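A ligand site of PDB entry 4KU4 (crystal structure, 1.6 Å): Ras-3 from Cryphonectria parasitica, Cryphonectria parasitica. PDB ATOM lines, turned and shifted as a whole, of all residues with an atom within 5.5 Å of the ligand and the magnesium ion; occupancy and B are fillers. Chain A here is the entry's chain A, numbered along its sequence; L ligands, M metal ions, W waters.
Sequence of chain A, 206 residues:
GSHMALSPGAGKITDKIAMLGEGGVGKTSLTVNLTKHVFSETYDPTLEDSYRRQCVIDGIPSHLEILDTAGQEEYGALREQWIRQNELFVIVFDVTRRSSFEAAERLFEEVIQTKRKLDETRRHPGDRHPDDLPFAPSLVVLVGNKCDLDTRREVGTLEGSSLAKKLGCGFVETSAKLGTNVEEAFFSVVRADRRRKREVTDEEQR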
ATOM      1  N   GLU A  22      -9.185  -8.835  27.646  1.00  0.00           N
ATOM      2  CA  GLU A  22     -10.241  -8.715  26.638  1.00  0.00           C
ATOM      3  C   GLU A  22      -9.884  -7.673  25.591  1.00  0.00           C
ATOM      4  O   GLU A  22      -8.992  -6.844  25.784  1.00  0.00           O
ATOM      5  CB  GLU A  22     -11.564  -8.334  27.284  1.00  0.00           C
ATOM      6  CG  GLU A  22     -12.233  -9.441  28.041  1.00  0.00           C
ATOM      7  CD  GLU A  22     -13.665  -9.095  28.406  1.00  0.00           C
ATOM      8  OE1 GLU A  22     -13.944  -7.908  28.688  1.00  0.00           O
ATOM      9  OE2 GLU A  22     -14.520 -10.006  28.380  1.00  0.00           O
ATOM     10  N   GLY A  23     -10.616  -7.693  24.478  1.00  0.00           N
ATOM     11  CA  GLY A  23     -10.435  -6.681  23.456  1.00  0.00           C
ATOM     12  C   GLY A  23     -10.711  -5.278  23.952  1.00  0.00           C
ATOM     13  O   GLY A  23     -11.649  -5.062  24.721  1.00  0.00           O
ATOM     14  N   GLY A  24      -9.890  -4.329  23.517  1.00  0.00           N
ATOM     15  CA  GLY A  24     -10.125  -2.931  23.790  1.00  0.00           C
ATOM     16  C   GLY A  24      -9.566  -2.415  25.102  1.00  0.00           C
ATOM     17  O   GLY A  24      -9.795  -1.270  25.435  1.00  0.00           O
ATOM     18  N   VAL A  25      -8.804  -3.241  25.836  1.00  0.00           N
ATOM     19  CA  VAL A  25      -8.345  -2.812  27.167  1.00  0.00           C
ATOM     20  C   VAL A  25      -7.072  -1.985  27.077  1.00  0.00           C
ATOM     21  O   VAL A  25      -6.757  -1.192  27.986  1.00  0.00           O
ATOM     22  CB  VAL A  25      -8.176  -3.984  28.158  1.00  0.00           C
ATOM     23  CG1 VAL A  25      -9.563  -4.604  28.523  1.00  0.00           C
ATOM     24  CG2 VAL A  25      -7.185  -5.018  27.631  1.00  0.00           C
ATOM     25  N   GLY A  26      -6.365  -2.147  25.970  1.00  0.00           N
ATOM     26  CA  GLY A  26      -5.151  -1.383  25.741  1.00  0.00           C
ATOM     27  C   GLY A  26      -3.896  -2.222  25.574  1.00  0.00           C
ATOM     28  O   GLY A  26      -2.796  -1.700  25.731  1.00  0.00           O
ATOM     29  N   LYS A  27      -4.043  -3.504  25.268  1.00  0.00           N
ATOM     30  CA  LYS A  27      -2.867  -4.378  25.102  1.00  0.00           C
ATOM     31  C   LYS A  27      -1.877  -3.851  24.055  1.00  0.00           C
ATOM     32  O   LYS A  27      -0.693  -3.615  24.359  1.00  0.00           O
ATOM     33  CB  LYS A  27      -3.293  -5.814  24.759  1.00  0.00           C
ATOM     34  CG  LYS A  27      -4.129  -6.514  25.833  1.00  0.00           C
ATOM     35  CD  LYS A  27      -4.444  -7.944  25.452  1.00  0.00           C
ATOM     36  CE  LYS A  27      -5.306  -8.041  24.181  1.00  0.00           C
ATOM     37  NZ  LYS A  27      -6.603  -7.333  24.373  1.00  0.00           N
ATOM     38  N   THR A  28      -2.360  -3.682  22.829  1.00  0.00           N
ATOM     39  CA  THR A  28      -1.512  -3.190  21.745  1.00  0.00           C
ATOM     40  C   THR A  28      -0.900  -1.828  22.054  1.00  0.00           C
ATOM     41  O   THR A  28       0.296  -1.613  21.828  1.00  0.00           O
ATOM     42  CB  THR A  28      -2.295  -3.097  20.429  1.00  0.00           C
ATOM     43  OG1 THR A  28      -2.766  -4.405  20.068  1.00  0.00           O
ATOM     44  CG2 THR A  28      -1.378  -2.561  19.311  1.00  0.00           C
ATOM     45  N   SER A  29      -1.726  -0.918  22.566  1.00  0.00           N
ATOM     46  CA  SER A  29      -1.285   0.442  22.905  1.00  0.00           C
ATOM     47  C   SER A  29      -0.156   0.428  23.937  1.00  0.00           C
ATOM     48  O   SER A  29       0.842   1.137  23.788  1.00  0.00           O
ATOM     49  CB  SER A  29      -2.474   1.286  23.393  1.00  0.00           C
ATOM     50  OG  SER A  29      -3.430   1.464  22.352  1.00  0.00           O
ATOM     51  N   LEU A  30      -0.298  -0.404  24.959  1.00  0.00           N
ATOM     52  CA  LEU A  30       0.733  -0.553  25.984  1.00  0.00           C
ATOM     53  C   LEU A  30       2.049  -1.045  25.380  1.00  0.00           C
ATOM     54  O   LEU A  30       3.119  -0.515  25.679  1.00  0.00           O
ATOM     55  CB  LEU A  30       0.276  -1.531  27.070  1.00  0.00           C
ATOM     56  CG  LEU A  30      -0.706  -0.997  28.110  1.00  0.00           C
ATOM     57  CD1 LEU A  30      -1.343  -2.160  28.851  1.00  0.00           C
ATOM     58  CD2 LEU A  30      -0.023  -0.052  29.076  1.00  0.00           C
ATOM     59  N   ASP A  44      -1.490  -0.414  14.866  1.00  0.00           N
ATOM     60  CA  ASP A  44      -2.464  -1.418  15.318  1.00  0.00           C
ATOM     61  C   ASP A  44      -2.838  -2.385  14.201  1.00  0.00           C
ATOM     62  O   ASP A  44      -3.968  -2.331  13.695  1.00  0.00           O
ATOM     63  CB  ASP A  44      -3.742  -0.756  15.818  1.00  0.00           C
ATOM     64  CG  ASP A  44      -4.722  -1.747  16.419  1.00  0.00           C
ATOM     65  OD1 ASP A  44      -4.281  -2.853  16.809  1.00  0.00           O
ATOM     66  OD2 ASP A  44      -5.938  -1.441  16.508  1.00  0.00           O
ATOM     67  N   GLU A  48      -1.887  -9.287  14.942  1.00  0.00           N
ATOM     68  CA  GLU A  48      -0.983  -8.847  16.015  1.00  0.00           C
ATOM     69  C   GLU A  48       0.478  -9.172  15.776  1.00  0.00           C
ATOM     70  O   GLU A  48       0.808 -10.190  15.170  1.00  0.00           O
ATOM     71  CB  GLU A  48      -1.378  -9.472  17.354  1.00  0.00           C
ATOM     72  CG  GLU A  48      -2.587  -8.838  17.973  1.00  0.00           C
ATOM     73  CD  GLU A  48      -3.870  -9.273  17.314  1.00  0.00           C
ATOM     74  OE1 GLU A  48      -3.895 -10.401  16.740  1.00  0.00           O
ATOM     75  OE2 GLU A  48      -4.831  -8.492  17.367  1.00  0.00           O
ATOM     76  N   ASP A  68       1.859  -9.731  21.681  1.00  0.00           N
ATOM     77  CA  ASP A  68       0.560  -9.072  21.703  1.00  0.00           C
ATOM     78  C   ASP A  68      -0.406 -10.140  21.224  1.00  0.00           C
ATOM     79  O   ASP A  68      -0.031 -11.014  20.427  1.00  0.00           O
ATOM     80  CB  ASP A  68       0.579  -7.856  20.762  1.00  0.00           C
ATOM     81  CG  ASP A  68      -0.651  -6.975  20.899  1.00  0.00           C
ATOM     82  OD1 ASP A  68      -1.432  -7.163  21.856  1.00  0.00           O
ATOM     83  OD2 ASP A  68      -0.838  -6.060  20.065  1.00  0.00           O
ATOM     84  N   THR A  69      -1.634 -10.106  21.740  1.00  0.00           N
ATOM     85  CA  THR A  69      -2.601 -11.160  21.453  1.00  0.00           C
ATOM     86  C   THR A  69      -3.984 -10.592  21.186  1.00  0.00           C
ATOM     87  O   THR A  69      -4.305  -9.467  21.560  1.00  0.00           O
ATOM     88  CB  THR A  69      -2.751 -12.157  22.629  1.00  0.00           C
ATOM     89  OG1 THR A  69      -3.264 -11.472  23.782  1.00  0.00           O
ATOM     90  CG2 THR A  69      -1.404 -12.815  22.967  1.00  0.00           C
ATOM     91  N   ALA A  70      -4.816 -11.407  20.554  1.00  0.00           N
ATOM     92  CA  ALA A  70      -6.189 -11.044  20.263  1.00  0.00           C
ATOM     93  C   ALA A  70      -6.823 -12.198  19.508  1.00  0.00           C
ATOM     94  O   ALA A  70      -6.149 -12.866  18.729  1.00  0.00           O
ATOM     95  CB  ALA A  70      -6.228  -9.786  19.432  1.00  0.00           C
ATOM     96  N   ASN A 145      -5.395  -0.353  33.068  1.00  0.00           N
ATOM     97  CA  ASN A 145      -5.039   0.623  32.043  1.00  0.00           C
ATOM     98  C   ASN A 145      -6.132   1.668  31.846  1.00  0.00           C
ATOM     99  O   ASN A 145      -7.261   1.483  32.320  1.00  0.00           O
ATOM    100  CB  ASN A 145      -4.733  -0.067  30.712  1.00  0.00           C
ATOM    101  CG  ASN A 145      -4.131   0.871  29.677  1.00  0.00           C
ATOM    102  OD1 ASN A 145      -3.242   1.675  29.996  1.00  0.00           O
ATOM    103  ND2 ASN A 145      -4.586   0.770  28.425  1.00  0.00           N
ATOM    104  N   LYS A 146      -5.775   2.751  31.172  1.00  0.00           N
ATOM    105  CA  LYS A 146      -6.645   3.905  30.928  1.00  0.00           C
ATOM    106  C   LYS A 146      -6.881   4.706  32.204  1.00  0.00           C
ATOM    107  O   LYS A 146      -7.967   5.228  32.429  1.00  0.00           O
ATOM    108  CB  LYS A 146      -7.968   3.490  30.263  1.00  0.00           C
ATOM    109  CG  LYS A 146      -7.855   2.440  29.162  1.00  0.00           C
ATOM    110  CD  LYS A 146      -8.995   2.564  28.163  1.00  0.00           C
ATOM    111  CE  LYS A 146      -8.925   1.439  27.115  1.00  0.00           C
ATOM    112  NZ  LYS A 146     -10.213   1.325  26.361  1.00  0.00           N
ATOM    113  N   CYS A 147      -5.852   4.804  33.044  1.00  0.00           N
ATOM    114  CA  CYS A 147      -6.025   5.522  34.303  1.00  0.00           C
ATOM    115  C   CYS A 147      -6.141   7.042  34.112  1.00  0.00           C
ATOM    116  O   CYS A 147      -6.513   7.755  35.032  1.00  0.00           O
ATOM    117  CB  CYS A 147      -4.910   5.188  35.389  1.00  0.00           C
ATOM    118  SG  CYS A 147      -3.235   5.721  34.904  1.00  0.00           S
ATOM    119  N   ASP A 148      -5.839   7.524  32.910  1.00  0.00           N
ATOM    120  CA  ASP A 148      -6.036   8.943  32.573  1.00  0.00           C
ATOM    121  C   ASP A 148      -7.535   9.247  32.499  1.00  0.00           C
ATOM    122  O   ASP A 148      -7.952  10.406  32.489  1.00  0.00           O
ATOM    123  CB  ASP A 148      -5.365   9.282  31.239  1.00  0.00           C
ATOM    124  CG  ASP A 148      -5.848   8.401  30.115  1.00  0.00           C
ATOM    125  OD1 ASP A 148      -5.469   7.214  30.093  1.00  0.00           O
ATOM    126  OD2 ASP A 148      -6.618   8.868  29.259  1.00  0.00           O
ATOM    127  N   LEU A 149      -8.346   8.195  32.452  1.00  0.00           N
ATOM    128  CA  LEU A 149      -9.800   8.314  32.369  1.00  0.00           C
ATOM    129  C   LEU A 149     -10.419   8.225  33.753  1.00  0.00           C
ATOM    130  O   LEU A 149     -11.414   7.522  33.969  1.00  0.00           O
ATOM    131  CB  LEU A 149     -10.385   7.238  31.437  1.00  0.00           C
ATOM    132  CG  LEU A 149      -9.930   7.397  29.975  1.00  0.00           C
ATOM    133  CD1 LEU A 149     -10.613   6.409  29.072  1.00  0.00           C
ATOM    134  CD2 LEU A 149     -10.192   8.823  29.522  1.00  0.00           C
ATOM    135  N   THR A 174      -1.842   2.084  34.746  1.00  0.00           N
ATOM    136  CA  THR A 174      -1.129   2.691  33.635  1.00  0.00           C
ATOM    137  C   THR A 174      -1.982   3.524  32.700  1.00  0.00           C
ATOM    138  O   THR A 174      -3.220   3.458  32.744  1.00  0.00           O
ATOM    139  CB  THR A 174      -0.545   1.565  32.690  1.00  0.00           C
ATOM    140  OG1 THR A 174      -1.613   0.767  32.164  1.00  0.00           O
ATOM    141  CG2 THR A 174       0.438   0.687  33.458  1.00  0.00           C
ATOM    142  N   SER A 175      -1.330   4.361  31.907  1.00  0.00           N
ATOM    143  CA  SER A 175      -2.021   5.046  30.814  1.00  0.00           C
ATOM    144  C   SER A 175      -1.145   4.874  29.588  1.00  0.00           C
ATOM    145  O   SER A 175      -0.118   5.521  29.459  1.00  0.00           O
ATOM    146  CB  SER A 175      -2.287   6.528  31.066  1.00  0.00           C
ATOM    147  OG  SER A 175      -2.844   7.128  29.898  1.00  0.00           O
ATOM    148  N   ALA A 176      -1.518   3.917  28.728  1.00  0.00           N
ATOM    149  CA  ALA A 176      -0.825   3.715  27.469  1.00  0.00           C
ATOM    150  C   ALA A 176      -0.794   4.986  26.656  1.00  0.00           C
ATOM    151  O   ALA A 176       0.130   5.223  25.879  1.00  0.00           O
ATOM    152  CB  ALA A 176      -1.502   2.601  26.668  1.00  0.00           C
ATOM    153  N   LYS A 177      -1.827   5.812  26.820  1.00  0.00           N
ATOM    154  CA  LYS A 177      -1.971   7.023  26.018  1.00  0.00           C
ATOM    155  C   LYS A 177      -0.939   8.056  26.446  1.00  0.00           C
ATOM    156  O   LYS A 177      -0.294   8.684  25.615  1.00  0.00           O
ATOM    157  CB  LYS A 177      -3.389   7.591  26.147  1.00  0.00           C
ATOM    158  CG  LYS A 177      -3.616   8.887  25.371  1.00  0.00           C
ATOM    159  CD  LYS A 177      -4.955   9.517  25.732  1.00  0.00           C
ATOM    160  CE  LYS A 177      -5.008  10.972  25.280  1.00  0.00           C
ATOM    161  NZ  LYS A 177      -6.224  11.694  25.730  1.00  0.00           N
ATOM    162  N   LEU A 178      -0.752   8.201  27.755  1.00  0.00           N
ATOM    163  CA  LEU A 178       0.198   9.192  28.270  1.00  0.00           C
ATOM    164  C   LEU A 178       1.576   8.608  28.570  1.00  0.00           C
ATOM    165  O   LEU A 178       2.528   9.358  28.784  1.00  0.00           O
ATOM    166  CB  LEU A 178      -0.378   9.918  29.489  1.00  0.00           C
ATOM    167  CG  LEU A 178      -1.630  10.743  29.157  1.00  0.00           C
ATOM    168  CD1 LEU A 178      -2.143  11.457  30.374  1.00  0.00           C
ATOM    169  CD2 LEU A 178      -1.298  11.730  28.049  1.00  0.00           C
HETATM  170  P1  LIG L   1      -6.512  -3.916  22.764  1.00  0.00           P
HETATM  171  O1  LIG L   1      -5.227  -4.183  22.001  1.00  0.00           O
HETATM  172  O2  LIG L   1      -6.399  -4.503  24.165  1.00  0.00           O
HETATM  173  O3  LIG L   1      -7.690  -4.524  22.029  1.00  0.00           O
HETATM  174  O4  LIG L   1      -6.708  -2.320  22.896  1.00  0.00           O
HETATM  175  P2  LIG L   1      -6.063  -1.158  21.942  1.00  0.00           P
HETATM  176  O5  LIG L   1      -4.599  -0.923  22.226  1.00  0.00           O
HETATM  177  O6  LIG L   1      -6.297  -1.407  20.477  1.00  0.00           O
HETATM  178  O7  LIG L   1      -6.858   0.146  22.430  1.00  0.00           O
HETATM  179  C1  LIG L   1      -8.284   0.162  22.314  1.00  0.00           C
HETATM  180  C2  LIG L   1      -8.735   1.605  22.428  1.00  0.00           C
HETATM  181  O8  LIG L   1      -8.344   2.058  23.706  1.00  0.00           O
HETATM  182  C3  LIG L   1      -8.061   2.522  21.425  1.00  0.00           C
HETATM  183  O9  LIG L   1      -9.004   3.507  20.962  1.00  0.00           O
HETATM  184  C4  LIG L   1      -6.983   3.198  22.236  1.00  0.00           C
HETATM  185  O10 LIG L   1      -6.671   4.504  21.739  1.00  0.00           O
HETATM  186  C5  LIG L   1      -7.628   3.263  23.606  1.00  0.00           C
HETATM  187  N1  LIG L   1      -6.647   3.254  24.711  1.00  0.00           N
HETATM  188  C6  LIG L   1      -5.731   2.305  24.975  1.00  0.00           C
HETATM  189  N2  LIG L   1      -5.025   2.621  26.090  1.00  0.00           N
HETATM  190  C7  LIG L   1      -5.508   3.783  26.553  1.00  0.00           C
HETATM  191  C8  LIG L   1      -5.226   4.673  27.683  1.00  0.00           C
HETATM  192  O11 LIG L   1      -4.332   4.396  28.504  1.00  0.00           O
HETATM  193  N3  LIG L   1      -5.972   5.788  27.818  1.00  0.00           N
HETATM  194  C9  LIG L   1      -6.934   6.118  26.957  1.00  0.00           C
HETATM  195  N4  LIG L   1      -7.619   7.265  27.181  1.00  0.00           N
HETATM  196  N5  LIG L   1      -7.252   5.347  25.893  1.00  0.00           N
HETATM  197  C10 LIG L   1      -6.578   4.196  25.647  1.00  0.00           C
HETATM  198 MG    MG M   1      -4.771  -5.282  20.173  1.00  0.00          MG
HETATM  199  O   HOH W   1      -3.978  -6.896  21.378  1.00  0.00           O
HETATM  200  O   HOH W   2      -8.428   5.779  19.635  1.00  0.00           O
HETATM  201  O   HOH W   3      -6.786  -6.180  20.180  1.00  0.00           O
HETATM  202  O   HOH W   4      -8.035   7.127  22.870  1.00  0.00           O
HETATM  203  O   HOH W   5      -8.077  -1.759  18.051  1.00  0.00           O
HETATM  204  O   HOH W   6      -9.173  -3.072  20.061  1.00  0.00           O
HETATM  205  O   HOH W   7      -9.066   8.680  25.100  1.00  0.00           O
HETATM  206  O   HOH W   8      -3.737   4.130  21.422  1.00  0.00           O
HETATM  207  O   HOH W   9     -11.412   2.987  19.809  1.00  0.00           O
HETATM  208  O   HOH W  10      -5.534  -3.582  19.022  1.00  0.00           O
HETATM  209  O   HOH W  11      -9.739   6.294  24.615  1.00  0.00           O
HETATM  210  O   HOH W  12      -4.331  -6.107  18.240  1.00  0.00           O
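ND2 of Asn 145 is in hydrogen-bond range of N2 of the ligand (3.0 Å).
An oxygen (O11) of the ligand sits at hydrogen-bond distance from the backbone NH (N) of Lys 177 (3.3 Å).
The backbone NH of Thr 28 sits close to an oxygen (O1) of the ligand, 3.0 Å away.
The side-chain carboxylate of Asp 148 lies within hydrogen-bond range of a nitrogen (N3) of the ligand (2.7 Å).
The side-chain amino group (NZ) of Lys 27 lies within salt-bridge range of an oxygen (O2) of the ligand (2.8 Å).
An oxygen (O5) of the ligand lies within hydrogen-bond range of the backbone NH (N) of Ser 29 (2.9 Å).
An oxygen (O8) of the ligand sits at hydrogen-bond distance from the side-chain amino group of Lys 146, 3.3 Å away.
An oxygen (O11) of the ligand sits close to the side-chain hydroxyl of Ser 175 (3.4 Å).
The backbone NH (N) of Lys 27 sits at hydrogen-bond distance from an oxygen (O2) of the ligand (2.8 Å).
An oxygen (O11) of the ligand sits close to the backbone NH (N) of Lys 146.
The backbone NH (N) of Gly 26 is in hydrogen-bond range of an oxygen (O2) of the ligand (3.0 Å).
The backbone NH (N) of Val 25 sits at hydrogen-bond distance from an oxygen (O2) of the ligand, 3.2 Å away.
O11 of the ligand lies within hydrogen-bond range of N of Ala 176 (2.9 Å).
The side-chain hydroxyl (OG) of Ser 29 is in hydrogen-bond range of an oxygen (O5) of the ligand, at 2.7 Å.
The backbone NH (N) of Gly 24 lies within hydrogen-bond range of an oxygen (O3) of the ligand, 2.7 Å away.
Water W10 bridges the side-chain carboxylate (OD1) of Asp 44 (2.6 Å) and an oxygen (O6) of the ligand (2.7 Å).
Water W1 lies within hydrogen-bond range of O of Thr 69 and OD1 of Asp 68.
Water W8 lies within hydrogen-bond range of the side-chain hydroxyl (OG) of Ser 29 (2.8 Å) and an oxygen (O10) of the ligand (3.0 Å).
Water W5 lies within hydrogen-bond range of OD2 of Asp 44 (2.7 Å) and O6 of the ligand (3.0 Å).
The side-chain hydroxyl (OG) of Ser 175 sits close to the backbone NH (N) of Lys 177, at 3.5 Å.
The side-chain amino group (NZ) of Lys 27 is in hydrogen-bond range of the backbone carbonyl oxygen (O) of Glu 22 (2.8 Å).
OD1 of Asp 148 is in hydrogen-bond range of OG of Ser 175.
The side-chain amide oxygen of Asn 145 is in hydrogen-bond range of the side-chain hydroxyl of Thr 174, at 2.9 Å.
N of Lys 146 lies within hydrogen-bond range of O of Thr 174, 3.1 Å away.
The side-chain amino group (NZ) of Lys 146 sits at hydrogen-bond distance from the backbone carbonyl oxygen (O) of Gly 24 (2.8 Å).
OG1 of Thr 28 lies close to OD2 of Asp 68 (2.5 Å).
N of Ala 176 is in hydrogen-bond range of OD1 of Asn 145.
One residue has an atom within 4 Å of the magnesium ion: Thr 28.
The nearest printed residue that does not touch the magnesium ion is Asp 68 (4.01 Å).
O of Glu 22 touches O2 of the ligand (3.9 Å).
C of Gly 23 touches O3 of the ligand (3.7 Å).
Asp 44 touches the ligand.
Leu 149 touches the ligand (CG to N4, 3.6 Å).
Hydrophobic or aromatic side chains that line the ligand: Val 25, Leu 149 and Ala 176.
The magnesium ion is bound by water W12, water W1, O1 of the ligand, water W10, OG1 of Thr 28 and water W3.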
